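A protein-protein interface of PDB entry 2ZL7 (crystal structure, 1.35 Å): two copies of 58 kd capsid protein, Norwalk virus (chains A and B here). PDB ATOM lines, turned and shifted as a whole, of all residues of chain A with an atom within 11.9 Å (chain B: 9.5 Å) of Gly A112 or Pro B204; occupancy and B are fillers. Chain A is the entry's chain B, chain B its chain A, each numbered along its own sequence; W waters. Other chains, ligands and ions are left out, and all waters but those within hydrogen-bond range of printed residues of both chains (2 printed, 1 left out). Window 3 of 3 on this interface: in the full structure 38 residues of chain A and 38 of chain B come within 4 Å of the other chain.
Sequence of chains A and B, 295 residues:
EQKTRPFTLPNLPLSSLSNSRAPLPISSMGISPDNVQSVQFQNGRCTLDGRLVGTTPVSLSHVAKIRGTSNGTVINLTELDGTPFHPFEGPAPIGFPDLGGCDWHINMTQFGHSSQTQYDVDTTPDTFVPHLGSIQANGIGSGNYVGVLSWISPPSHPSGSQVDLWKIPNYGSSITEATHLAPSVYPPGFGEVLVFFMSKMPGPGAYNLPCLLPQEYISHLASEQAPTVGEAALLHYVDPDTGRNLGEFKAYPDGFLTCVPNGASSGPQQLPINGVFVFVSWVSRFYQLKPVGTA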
ATOM      1  N   ARG A  67       0.073  -0.586  -3.828  1.00  0.00           N
ATOM      2  CA  ARG A  67       0.843  -1.536  -3.030  1.00  0.00           C
ATOM      3  C   ARG A  67       0.682  -1.131  -1.585  1.00  0.00           C
ATOM      4  O   ARG A  67       0.778   0.033  -1.258  1.00  0.00           O
ATOM      5  CB  ARG A  67       2.323  -1.508  -3.411  1.00  0.00           C
ATOM      6  CG  ARG A  67       3.186  -2.459  -2.568  1.00  0.00           C
ATOM      7  CD  ARG A  67       3.446  -3.743  -3.238  1.00  0.00           C
ATOM      8  NE  ARG A  67       4.179  -4.712  -2.417  1.00  0.00           N
ATOM      9  CZ  ARG A  67       5.489  -4.962  -2.479  1.00  0.00           C
ATOM     10  NH1 ARG A  67       6.323  -4.328  -3.303  1.00  0.00           N
ATOM     11  NH2 ARG A  67       5.981  -5.917  -1.698  1.00  0.00           N
ATOM     12  N   MET A 108      -6.044  -7.915  -6.558  1.00  0.00           N
ATOM     13  CA  MET A 108      -4.959  -7.975  -5.586  1.00  0.00           C
ATOM     14  C   MET A 108      -4.256  -9.312  -5.623  1.00  0.00           C
ATOM     15  O   MET A 108      -4.905 -10.359  -5.554  1.00  0.00           O
ATOM     16  CB  MET A 108      -5.526  -7.768  -4.180  1.00  0.00           C
ATOM     17  CG  MET A 108      -6.305  -6.495  -4.004  1.00  0.00           C
ATOM     18  SD  MET A 108      -5.244  -5.037  -3.840  1.00  0.00           S
ATOM     19  CE  MET A 108      -5.160  -4.867  -2.055  1.00  0.00           C
ATOM     20  N   THR A 109      -2.937  -9.285  -5.767  1.00  0.00           N
ATOM     21  CA  THR A 109      -2.134 -10.489  -5.698  1.00  0.00           C
ATOM     22  C   THR A 109      -1.024 -10.302  -4.680  1.00  0.00           C
ATOM     23  O   THR A 109      -0.835  -9.207  -4.138  1.00  0.00           O
ATOM     24  CB  THR A 109      -1.538 -10.836  -7.064  1.00  0.00           C
ATOM     25  OG1 THR A 109      -0.853  -9.683  -7.569  1.00  0.00           O
ATOM     26  CG2 THR A 109      -2.624 -11.295  -8.037  1.00  0.00           C
ATOM     27  N   GLN A 110      -0.300 -11.384  -4.413  1.00  0.00           N
ATOM     28  CA  GLN A 110       0.746 -11.366  -3.392  1.00  0.00           C
ATOM     29  C   GLN A 110       1.964 -12.119  -3.811  1.00  0.00           C
ATOM     30  O   GLN A 110       1.863 -13.208  -4.340  1.00  0.00           O
ATOM     31  CB  GLN A 110       0.254 -12.007  -2.107  1.00  0.00           C
ATOM     32  CG  GLN A 110      -0.992 -11.397  -1.562  1.00  0.00           C
ATOM     33  CD  GLN A 110      -1.385 -12.041  -0.254  1.00  0.00           C
ATOM     34  OE1 GLN A 110      -1.989 -13.107  -0.247  1.00  0.00           O
ATOM     35  NE2 GLN A 110      -1.067 -11.379   0.862  1.00  0.00           N
ATOM     36  N   PHE A 111       3.127 -11.567  -3.515  1.00  0.00           N
ATOM     37  CA  PHE A 111       4.354 -12.300  -3.725  1.00  0.00           C
ATOM     38  C   PHE A 111       4.436 -13.416  -2.694  1.00  0.00           C
ATOM     39  O   PHE A 111       4.282 -13.173  -1.500  1.00  0.00           O
ATOM     40  CB  PHE A 111       5.555 -11.373  -3.583  1.00  0.00           C
ATOM     41  CG  PHE A 111       5.548 -10.243  -4.561  1.00  0.00           C
ATOM     42  CD1 PHE A 111       5.570 -10.493  -5.916  1.00  0.00           C
ATOM     43  CD2 PHE A 111       5.535  -8.929  -4.128  1.00  0.00           C
ATOM     44  CE1 PHE A 111       5.537  -9.460  -6.816  1.00  0.00           C
ATOM     45  CE2 PHE A 111       5.534  -7.891  -5.036  1.00  0.00           C
ATOM     46  CZ  PHE A 111       5.529  -8.178  -6.388  1.00  0.00           C
ATOM     47  N   GLY A 112       4.615 -14.642  -3.151  1.00  0.00           N
ATOM     48  CA  GLY A 112       4.752 -15.762  -2.252  1.00  0.00           C
ATOM     49  C   GLY A 112       3.459 -16.449  -1.856  1.00  0.00           C
ATOM     50  O   GLY A 112       3.502 -17.446  -1.125  1.00  0.00           O
ATOM     51  N   HIS A 113       2.308 -15.961  -2.324  1.00  0.00           N
ATOM     52  CA  HIS A 113       1.035 -16.627  -2.062  1.00  0.00           C
ATOM     53  C   HIS A 113       0.273 -16.893  -3.344  1.00  0.00           C
ATOM     54  O   HIS A 113       0.406 -16.154  -4.327  1.00  0.00           O
ATOM     55  CB  HIS A 113       0.165 -15.780  -1.149  1.00  0.00           C
ATOM     56  CG  HIS A 113       0.833 -15.413   0.135  1.00  0.00           C
ATOM     57  ND1 HIS A 113       0.760 -16.203   1.263  1.00  0.00           N
ATOM     58  CD2 HIS A 113       1.622 -14.365   0.457  1.00  0.00           C
ATOM     59  CE1 HIS A 113       1.450 -15.634   2.236  1.00  0.00           C
ATOM     60  NE2 HIS A 113       1.981 -14.517   1.774  1.00  0.00           N
ATOM     61  N   SER A 114      -0.518 -17.957  -3.328  1.00  0.00           N
ATOM     62  CA  SER A 114      -1.487 -18.214  -4.363  1.00  0.00           C
ATOM     63  C   SER A 114      -2.617 -17.197  -4.285  1.00  0.00           C
ATOM     64  O   SER A 114      -2.780 -16.473  -3.288  1.00  0.00           O
ATOM     65  CB  SER A 114      -2.094 -19.612  -4.194  1.00  0.00           C
ATOM     66  OG  SER A 114      -1.108 -20.615  -4.282  1.00  0.00           O
ATOM     67  N   SER A 115      -3.388 -17.170  -5.362  1.00  0.00           N
ATOM     68  CA  SER A 115      -4.719 -16.564  -5.430  1.00  0.00           C
ATOM     69  C   SER A 115      -4.714 -15.074  -5.737  1.00  0.00           C
ATOM     70  O   SER A 115      -3.691 -14.385  -5.640  1.00  0.00           O
ATOM     71  CB  SER A 115      -5.531 -16.807  -4.149  1.00  0.00           C
ATOM     72  OG  SER A 115      -5.446 -18.174  -3.753  1.00  0.00           O
ATOM     73  N   GLN A 116      -5.876 -14.600  -6.156  1.00  0.00           N
ATOM     74  CA  GLN A 116      -6.124 -13.194  -6.345  1.00  0.00           C
ATOM     75  C   GLN A 116      -7.402 -12.863  -5.598  1.00  0.00           C
ATOM     76  O   GLN A 116      -8.242 -13.753  -5.362  1.00  0.00           O
ATOM     77  CB  GLN A 116      -6.252 -12.841  -7.827  1.00  0.00           C
ATOM     78  CG  GLN A 116      -7.487 -13.427  -8.511  1.00  0.00           C
ATOM     79  CD  GLN A 116      -7.566 -13.109  -9.986  1.00  0.00           C
ATOM     80  OE1 GLN A 116      -6.528 -12.888 -10.632  1.00  0.00           O
ATOM     81  NE2 GLN A 116      -8.773 -13.073 -10.529  1.00  0.00           N
ATOM     82  N   SER A 142      -5.499  -9.263   6.344  1.00  0.00           N
ATOM     83  CA  SER A 142      -4.144  -8.844   6.625  1.00  0.00           C
ATOM     84  C   SER A 142      -3.164  -9.471   5.665  1.00  0.00           C
ATOM     85  O   SER A 142      -3.263 -10.645   5.322  1.00  0.00           O
ATOM     86  CB  SER A 142      -3.772  -9.217   8.059  1.00  0.00           C
ATOM     87  OG  SER A 142      -4.575  -8.474   8.950  1.00  0.00           O
ATOM     88  N   GLY A 143      -2.214  -8.655   5.216  1.00  0.00           N
ATOM     89  CA  GLY A 143      -1.175  -9.115   4.326  1.00  0.00           C
ATOM     90  C   GLY A 143      -0.686  -7.978   3.459  1.00  0.00           C
ATOM     91  O   GLY A 143      -1.273  -6.895   3.469  1.00  0.00           O
ATOM     92  N   ASN A 144       0.387  -8.241   2.721  1.00  0.00           N
ATOM     93  CA  ASN A 144       0.916  -7.282   1.755  1.00  0.00           C
ATOM     94  C   ASN A 144       0.451  -7.679   0.385  1.00  0.00           C
ATOM     95  O   ASN A 144       0.478  -8.856   0.055  1.00  0.00           O
ATOM     96  CB  ASN A 144       2.440  -7.252   1.777  1.00  0.00           C
ATOM     97  CG  ASN A 144       3.003  -6.159   0.892  1.00  0.00           C
ATOM     98  OD1 ASN A 144       3.351  -6.414  -0.248  1.00  0.00           O
ATOM     99  ND2 ASN A 144       3.043  -4.939   1.392  1.00  0.00           N
ATOM    100  N   TYR A 145      -0.028  -6.695  -0.370  1.00  0.00           N
ATOM    101  CA  TYR A 145      -0.577  -6.917  -1.704  1.00  0.00           C
ATOM    102  C   TYR A 145      -0.059  -5.916  -2.715  1.00  0.00           C
ATOM    103  O   TYR A 145       0.229  -4.769  -2.365  1.00  0.00           O
ATOM    104  CB  TYR A 145      -2.091  -6.730  -1.685  1.00  0.00           C
ATOM    105  CG  TYR A 145      -2.846  -7.645  -0.737  1.00  0.00           C
ATOM    106  CD1 TYR A 145      -3.416  -8.824  -1.181  1.00  0.00           C
ATOM    107  CD2 TYR A 145      -2.990  -7.314   0.594  1.00  0.00           C
ATOM    108  CE1 TYR A 145      -4.118  -9.646  -0.322  1.00  0.00           C
ATOM    109  CE2 TYR A 145      -3.689  -8.128   1.445  1.00  0.00           C
ATOM    110  CZ  TYR A 145      -4.228  -9.295   0.986  1.00  0.00           C
ATOM    111  OH  TYR A 145      -4.933 -10.098   1.850  1.00  0.00           O
ATOM    112  N   VAL A 146      -0.016  -6.346  -3.970  1.00  0.00           N
ATOM    113  CA  VAL A 146       0.018  -5.438  -5.117  1.00  0.00           C
ATOM    114  C   VAL A 146      -1.328  -5.556  -5.812  1.00  0.00           C
ATOM    115  O   VAL A 146      -1.838  -6.662  -5.982  1.00  0.00           O
ATOM    116  CB  VAL A 146       1.141  -5.763  -6.080  1.00  0.00           C
ATOM    117  CG1 VAL A 146       1.114  -4.816  -7.296  1.00  0.00           C
ATOM    118  CG2 VAL A 146       2.452  -5.670  -5.382  1.00  0.00           C
ATOM    119  N   CYS B 102       4.954 -23.436 -16.082  1.00  0.00           N
ATOM    120  CA  CYS B 102       4.057 -23.016 -15.026  1.00  0.00           C
ATOM    121  C   CYS B 102       2.604 -23.128 -15.486  1.00  0.00           C
ATOM    122  O   CYS B 102       2.336 -23.191 -16.690  1.00  0.00           O
ATOM    123  CB  CYS B 102       4.357 -21.566 -14.593  1.00  0.00           C
ATOM    124  SG  CYS B 102       4.136 -20.302 -15.881  1.00  0.00           S
ATOM    125  N   ASP B 103       1.678 -23.114 -14.537  1.00  0.00           N
ATOM    126  CA  ASP B 103       0.277 -22.856 -14.834  1.00  0.00           C
ATOM    127  C   ASP B 103       0.047 -21.357 -14.721  1.00  0.00           C
ATOM    128  O   ASP B 103       0.690 -20.671 -13.912  1.00  0.00           O
ATOM    129  CB  ASP B 103      -0.662 -23.550 -13.842  1.00  0.00           C
ATOM    130  CG  ASP B 103      -0.918 -25.020 -14.152  1.00  0.00           C
ATOM    131  OD1 ASP B 103      -0.254 -25.655 -14.999  1.00  0.00           O
ATOM    132  OD2 ASP B 103      -1.828 -25.548 -13.463  1.00  0.00           O
ATOM    133  N   HIS B 105      -2.697 -18.068 -14.163  1.00  0.00           N
ATOM    134  CA  HIS B 105      -3.973 -17.637 -13.613  1.00  0.00           C
ATOM    135  C   HIS B 105      -4.235 -16.258 -14.179  1.00  0.00           C
ATOM    136  O   HIS B 105      -3.480 -15.319 -13.914  1.00  0.00           O
ATOM    137  CB  HIS B 105      -3.912 -17.720 -12.090  1.00  0.00           C
ATOM    138  CG  HIS B 105      -3.600 -19.107 -11.635  1.00  0.00           C
ATOM    139  ND1 HIS B 105      -2.338 -19.551 -11.303  1.00  0.00           N
ATOM    140  CD2 HIS B 105      -4.405 -20.194 -11.601  1.00  0.00           C
ATOM    141  CE1 HIS B 105      -2.393 -20.852 -11.050  1.00  0.00           C
ATOM    142  NE2 HIS B 105      -3.637 -21.256 -11.204  1.00  0.00           N
ATOM    143  N   SER B 150      -2.219 -12.762 -14.206  1.00  0.00           N
ATOM    144  CA  SER B 150      -2.243 -12.185 -12.860  1.00  0.00           C
ATOM    145  C   SER B 150      -1.215 -12.842 -11.920  1.00  0.00           C
ATOM    146  O   SER B 150      -0.486 -12.147 -11.214  1.00  0.00           O
ATOM    147  CB  SER B 150      -3.658 -12.297 -12.301  1.00  0.00           C
ATOM    148  OG  SER B 150      -3.686 -11.888 -10.962  1.00  0.00           O
ATOM    149  N   TRP B 151      -1.172 -14.166 -11.892  1.00  0.00           N
ATOM    150  CA  TRP B 151      -0.206 -14.883 -11.063  1.00  0.00           C
ATOM    151  C   TRP B 151       0.014 -16.259 -11.663  1.00  0.00           C
ATOM    152  O   TRP B 151      -0.735 -16.684 -12.572  1.00  0.00           O
ATOM    153  CB  TRP B 151      -0.664 -14.947  -9.589  1.00  0.00           C
ATOM    154  CG  TRP B 151      -2.002 -15.621  -9.348  1.00  0.00           C
ATOM    155  CD1 TRP B 151      -3.226 -15.099  -9.553  1.00  0.00           C
ATOM    156  CD2 TRP B 151      -2.201 -16.944  -8.842  1.00  0.00           C
ATOM    157  NE1 TRP B 151      -4.205 -16.022  -9.219  1.00  0.00           N
ATOM    158  CE2 TRP B 151      -3.591 -17.154  -8.765  1.00  0.00           C
ATOM    159  CE3 TRP B 151      -1.343 -17.961  -8.414  1.00  0.00           C
ATOM    160  CZ2 TRP B 151      -4.141 -18.354  -8.298  1.00  0.00           C
ATOM    161  CZ3 TRP B 151      -1.897 -19.152  -7.950  1.00  0.00           C
ATOM    162  CH2 TRP B 151      -3.279 -19.335  -7.906  1.00  0.00           C
ATOM    163  N   ILE B 152       1.070 -16.941 -11.218  1.00  0.00           N
ATOM    164  CA  ILE B 152       1.425 -18.255 -11.756  1.00  0.00           C
ATOM    165  C   ILE B 152       1.634 -19.250 -10.630  1.00  0.00           C
ATOM    166  O   ILE B 152       1.749 -18.857  -9.465  1.00  0.00           O
ATOM    167  CB  ILE B 152       2.698 -18.234 -12.631  1.00  0.00           C
ATOM    168  CG1 ILE B 152       3.923 -17.905 -11.780  1.00  0.00           C
ATOM    169  CG2 ILE B 152       2.536 -17.247 -13.807  1.00  0.00           C
ATOM    170  CD1 ILE B 152       5.207 -18.085 -12.491  1.00  0.00           C
ATOM    171  N   SER B 153       1.664 -20.533 -10.984  1.00  0.00           N
ATOM    172  CA  SER B 153       1.907 -21.573  -9.989  1.00  0.00           C
ATOM    173  C   SER B 153       2.589 -22.716 -10.706  1.00  0.00           C
ATOM    174  O   SER B 153       2.740 -22.690 -11.921  1.00  0.00           O
ATOM    175  CB  SER B 153       0.578 -21.994  -9.366  1.00  0.00           C
ATOM    176  OG  SER B 153      -0.291 -22.488 -10.360  1.00  0.00           O
ATOM    177  N   PRO B 154       3.054 -23.742  -9.963  1.00  0.00           N
ATOM    178  CA  PRO B 154       3.701 -24.866 -10.633  1.00  0.00           C
ATOM    179  C   PRO B 154       2.824 -25.548 -11.693  1.00  0.00           C
ATOM    180  O   PRO B 154       1.600 -25.565 -11.567  1.00  0.00           O
ATOM    181  CB  PRO B 154       4.046 -25.806  -9.470  1.00  0.00           C
ATOM    182  CG  PRO B 154       4.184 -24.892  -8.297  1.00  0.00           C
ATOM    183  CD  PRO B 154       3.108 -23.873  -8.494  1.00  0.00           C
ATOM    184  N   PRO B 155       3.457 -26.095 -12.741  1.00  0.00           N
ATOM    185  CA  PRO B 155       2.669 -26.761 -13.773  1.00  0.00           C
ATOM    186  C   PRO B 155       1.860 -27.912 -13.211  1.00  0.00           C
ATOM    187  O   PRO B 155       2.348 -28.655 -12.346  1.00  0.00           O
ATOM    188  CB  PRO B 155       3.722 -27.315 -14.743  1.00  0.00           C
ATOM    189  CG  PRO B 155       4.984 -26.659 -14.418  1.00  0.00           C
ATOM    190  CD  PRO B 155       4.899 -26.184 -12.998  1.00  0.00           C
ATOM    191  N   GLN B 162       8.812 -28.274 -11.261  1.00  0.00           N
ATOM    192  CA  GLN B 162       9.199 -26.966 -10.743  1.00  0.00           C
ATOM    193  C   GLN B 162       8.659 -25.880 -11.664  1.00  0.00           C
ATOM    194  O   GLN B 162       8.181 -26.161 -12.782  1.00  0.00           O
ATOM    195  CB  GLN B 162      10.719 -26.848 -10.680  1.00  0.00           C
ATOM    196  CG  GLN B 162      11.402 -27.979  -9.905  1.00  0.00           C
ATOM    197  CD  GLN B 162      11.064 -27.945  -8.436  1.00  0.00           C
ATOM    198  OE1 GLN B 162      11.078 -26.890  -7.801  1.00  0.00           O
ATOM    199  NE2 GLN B 162      10.768 -29.109  -7.869  1.00  0.00           N
ATOM    200  N   VAL B 163       8.727 -24.641 -11.200  1.00  0.00           N
ATOM    201  CA  VAL B 163       8.435 -23.484 -12.053  1.00  0.00           C
ATOM    202  C   VAL B 163       9.721 -23.127 -12.767  1.00  0.00           C
ATOM    203  O   VAL B 163      10.743 -22.853 -12.141  1.00  0.00           O
ATOM    204  CB  VAL B 163       7.933 -22.309 -11.218  1.00  0.00           C
ATOM    205  CG1 VAL B 163       7.926 -21.012 -12.040  1.00  0.00           C
ATOM    206  CG2 VAL B 163       6.550 -22.604 -10.666  1.00  0.00           C
ATOM    207  N   LYS B 200       9.737  -9.823 -10.258  1.00  0.00           N
ATOM    208  CA  LYS B 200       9.031 -10.695  -9.321  1.00  0.00           C
ATOM    209  C   LYS B 200       7.615 -10.946  -9.813  1.00  0.00           C
ATOM    210  O   LYS B 200       6.867 -10.004 -10.053  1.00  0.00           O
ATOM    211  CB  LYS B 200       8.983 -10.037  -7.939  1.00  0.00           C
ATOM    212  CG  LYS B 200      10.355  -9.837  -7.279  1.00  0.00           C
ATOM    213  CD  LYS B 200      10.311  -8.833  -6.118  1.00  0.00           C
ATOM    214  CE  LYS B 200       9.272  -9.190  -5.079  1.00  0.00           C
ATOM    215  NZ  LYS B 200       9.310  -8.315  -3.857  1.00  0.00           N
ATOM    216  N   MET B 201       7.233 -12.214  -9.935  1.00  0.00           N
ATOM    217  CA  MET B 201       5.880 -12.609 -10.395  1.00  0.00           C
ATOM    218  C   MET B 201       5.114 -13.196  -9.208  1.00  0.00           C
ATOM    219  O   MET B 201       5.597 -14.143  -8.587  1.00  0.00           O
ATOM    220  CB  MET B 201       5.979 -13.664 -11.510  1.00  0.00           C
ATOM    221  CG  MET B 201       4.683 -14.361 -11.875  1.00  0.00           C
ATOM    222  SD  MET B 201       3.410 -13.284 -12.524  1.00  0.00           S
ATOM    223  CE  MET B 201       3.969 -13.155 -14.205  1.00  0.00           C
ATOM    224  N   PRO B 202       3.924 -12.657  -8.892  1.00  0.00           N
ATOM    225  CA  PRO B 202       3.164 -13.259  -7.808  1.00  0.00           C
ATOM    226  C   PRO B 202       2.770 -14.714  -8.047  1.00  0.00           C
ATOM    227  O   PRO B 202       2.665 -15.199  -9.183  1.00  0.00           O
ATOM    228  CB  PRO B 202       1.914 -12.376  -7.685  1.00  0.00           C
ATOM    229  CG  PRO B 202       1.868 -11.592  -8.870  1.00  0.00           C
ATOM    230  CD  PRO B 202       3.264 -11.453  -9.417  1.00  0.00           C
ATOM    231  N   GLY B 203       2.519 -15.377  -6.927  1.00  0.00           N
ATOM    232  CA  GLY B 203       2.210 -16.791  -6.864  1.00  0.00           C
ATOM    233  C   GLY B 203       2.900 -17.401  -5.661  1.00  0.00           C
ATOM    234  O   GLY B 203       3.635 -16.709  -4.953  1.00  0.00           O
ATOM    235  N   PRO B 204       2.649 -18.694  -5.421  1.00  0.00           N
ATOM    236  CA  PRO B 204       3.129 -19.384  -4.206  1.00  0.00           C
ATOM    237  C   PRO B 204       4.588 -19.818  -4.237  1.00  0.00           C
ATOM    238  O   PRO B 204       4.929 -20.977  -3.916  1.00  0.00           O
ATOM    239  CB  PRO B 204       2.233 -20.605  -4.158  1.00  0.00           C
ATOM    240  CG  PRO B 204       1.970 -20.925  -5.602  1.00  0.00           C
ATOM    241  CD  PRO B 204       1.791 -19.572  -6.235  1.00  0.00           C
ATOM    242  N   GLY B 205       5.460 -18.921  -4.620  1.00  0.00           N
ATOM    243  CA  GLY B 205       6.886 -19.168  -4.627  1.00  0.00           C
ATOM    244  C   GLY B 205       7.611 -17.891  -4.978  1.00  0.00           C
ATOM    245  O   GLY B 205       6.974 -16.882  -5.296  1.00  0.00           O
ATOM    246  N   ALA B 206       8.926 -17.919  -4.927  1.00  0.00           N
ATOM    247  CA  ALA B 206       9.738 -16.754  -5.223  1.00  0.00           C
ATOM    248  C   ALA B 206      10.087 -16.767  -6.696  1.00  0.00           C
ATOM    249  O   ALA B 206      11.195 -17.110  -7.104  1.00  0.00           O
ATOM    250  CB  ALA B 206      10.981 -16.731  -4.362  1.00  0.00           C
ATOM    251  N   TYR B 207       9.112 -16.392  -7.511  1.00  0.00           N
ATOM    252  CA  TYR B 207       9.228 -16.532  -8.952  1.00  0.00           C
ATOM    253  C   TYR B 207       9.819 -15.275  -9.547  1.00  0.00           C
ATOM    254  O   TYR B 207       9.388 -14.173  -9.222  1.00  0.00           O
ATOM    255  CB  TYR B 207       7.859 -16.813  -9.563  1.00  0.00           C
ATOM    256  CG  TYR B 207       7.136 -18.004  -8.980  1.00  0.00           C
ATOM    257  CD1 TYR B 207       7.818 -19.189  -8.687  1.00  0.00           C
ATOM    258  CD2 TYR B 207       5.771 -17.960  -8.734  1.00  0.00           C
ATOM    259  CE1 TYR B 207       7.147 -20.278  -8.170  1.00  0.00           C
ATOM    260  CE2 TYR B 207       5.107 -19.059  -8.218  1.00  0.00           C
ATOM    261  CZ  TYR B 207       5.805 -20.201  -7.923  1.00  0.00           C
ATOM    262  OH  TYR B 207       5.108 -21.272  -7.407  1.00  0.00           O
HETATM  263  O   HOH W   1       8.997  -6.879  -1.464  1.00  0.00           O
HETATM  264  O   HOH W   2       8.793  -5.684  -4.743  1.00  0.00           O
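OG of Ser B150 is in hydrogen-bond range of OE1 of Gln A116 (3.0 Å). N of Gly B203 sits at hydrogen-bond distance from O of Gln A110 (3.4 Å). N of His A113 is in hydrogen-bond range of O of Gly B203 (3.0 Å). The backbone carbonyl oxygen of Gly B203 lies within hydrogen-bond range of the backbone NH of Gly A112 (2.9 Å).
The backbone NH (N) of Ser B150 lies within hydrogen-bond range of the backbone carbonyl oxygen (O) of His B105. The backbone NH (N) of Thr A109 lies within hydrogen-bond range of the backbone carbonyl oxygen (O) of Val A146 (2.9 Å). The backbone carbonyl oxygen of Pro B202 is in hydrogen-bond range of the backbone NH of Ile B152. The backbone carbonyl oxygen (O) of Trp B151 sits at hydrogen-bond distance from the backbone NH (N) of His B105. NE2 of Gln A110 lies within hydrogen-bond range of O of Asn A144 (3.1 Å).
Among the printed residues, pairs that only touch across the chains: Thr A109 with Ser B150 (3.2 Å), Ser A115 with Trp B151 (3.3 Å), Ser A114 with Pro B204 (3.3 Å), Gln A110 with Pro B202 (3.4 Å), Phe A111 with Lys B200 (3.5 Å), His A113 with Pro B204 (3.6 Å), Thr A109 with Pro B202 (3.6 Å), Gly A112 with Pro B204 (3.7 Å), Ser A114 with Trp B151 (3.7 Å), Gln A116 with Trp B151 (3.8 Å), Gly A112 with Gly B205 (3.9 Å) and Phe A111 with Pro B202 (3.99 Å).
Of the printed residues of chain B, Thr A109 touches Ser B150 and Pro B202. Of the printed residues of chain B, Gln A110 touches Pro B202 and Gly B203. Gly A112 touches just these residues of chain B: Gly B203 (2.9 Å), Pro B204 (3.7 Å) and Gly B205 (3.9 Å). Printed residues of chain B within 4 Å of His A113: Gly B203 and Pro B204. Of the printed residues of chain B, Ser A115 touches Trp B151. Of the printed residues of chain B, Gln A116 touches Ser B150 and Trp B151. Of the printed residues of chain A, Trp B151 touches Ser A114 (3.7 Å), Ser A115 (3.3 Å) and Gln A116 (3.8 Å). No residue of chain A comes within 4 Å of Ser B153. No residue of chain A comes within 4 Å of Pro B154. Of chain A, only Gly A112, His A113 and Ser A114 come within 4 Å of Pro B204. Gly B205 touches one residue of chain A. No residue of chain A comes within 4 Å of Ala B206. The nearest residue of chain B that does not touch Gly A112 is Pro B202 (5.1 Å). The nearest printed residue of chain A that does not touch Pro B202 is His A113 (4.6 Å).
Of the 19 printed residues of chain B, 7 touch a printed residue of chain A. Among the printed residues, 16 pairs touch across the chains. Among the printed residues, no Asp or Glu carboxylate lies within 4 Å of a Lys or Arg side-chain nitrogen of the other chain.
No position is printed for both chains. Of the 16 pairs that touch across the chains among the printed residues, none has its exchanged pair printed and touching as well.
Water W1 lies within hydrogen-bond range of the side-chain amino group (NZ) of Lys B200 and the guanidinium group (NH2) of Arg A67. Water W2 lies within hydrogen-bond range of the side-chain amino group of Lys B200 (2.8 Å) and the guanidinium group of Arg A67 (3.2 Å).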
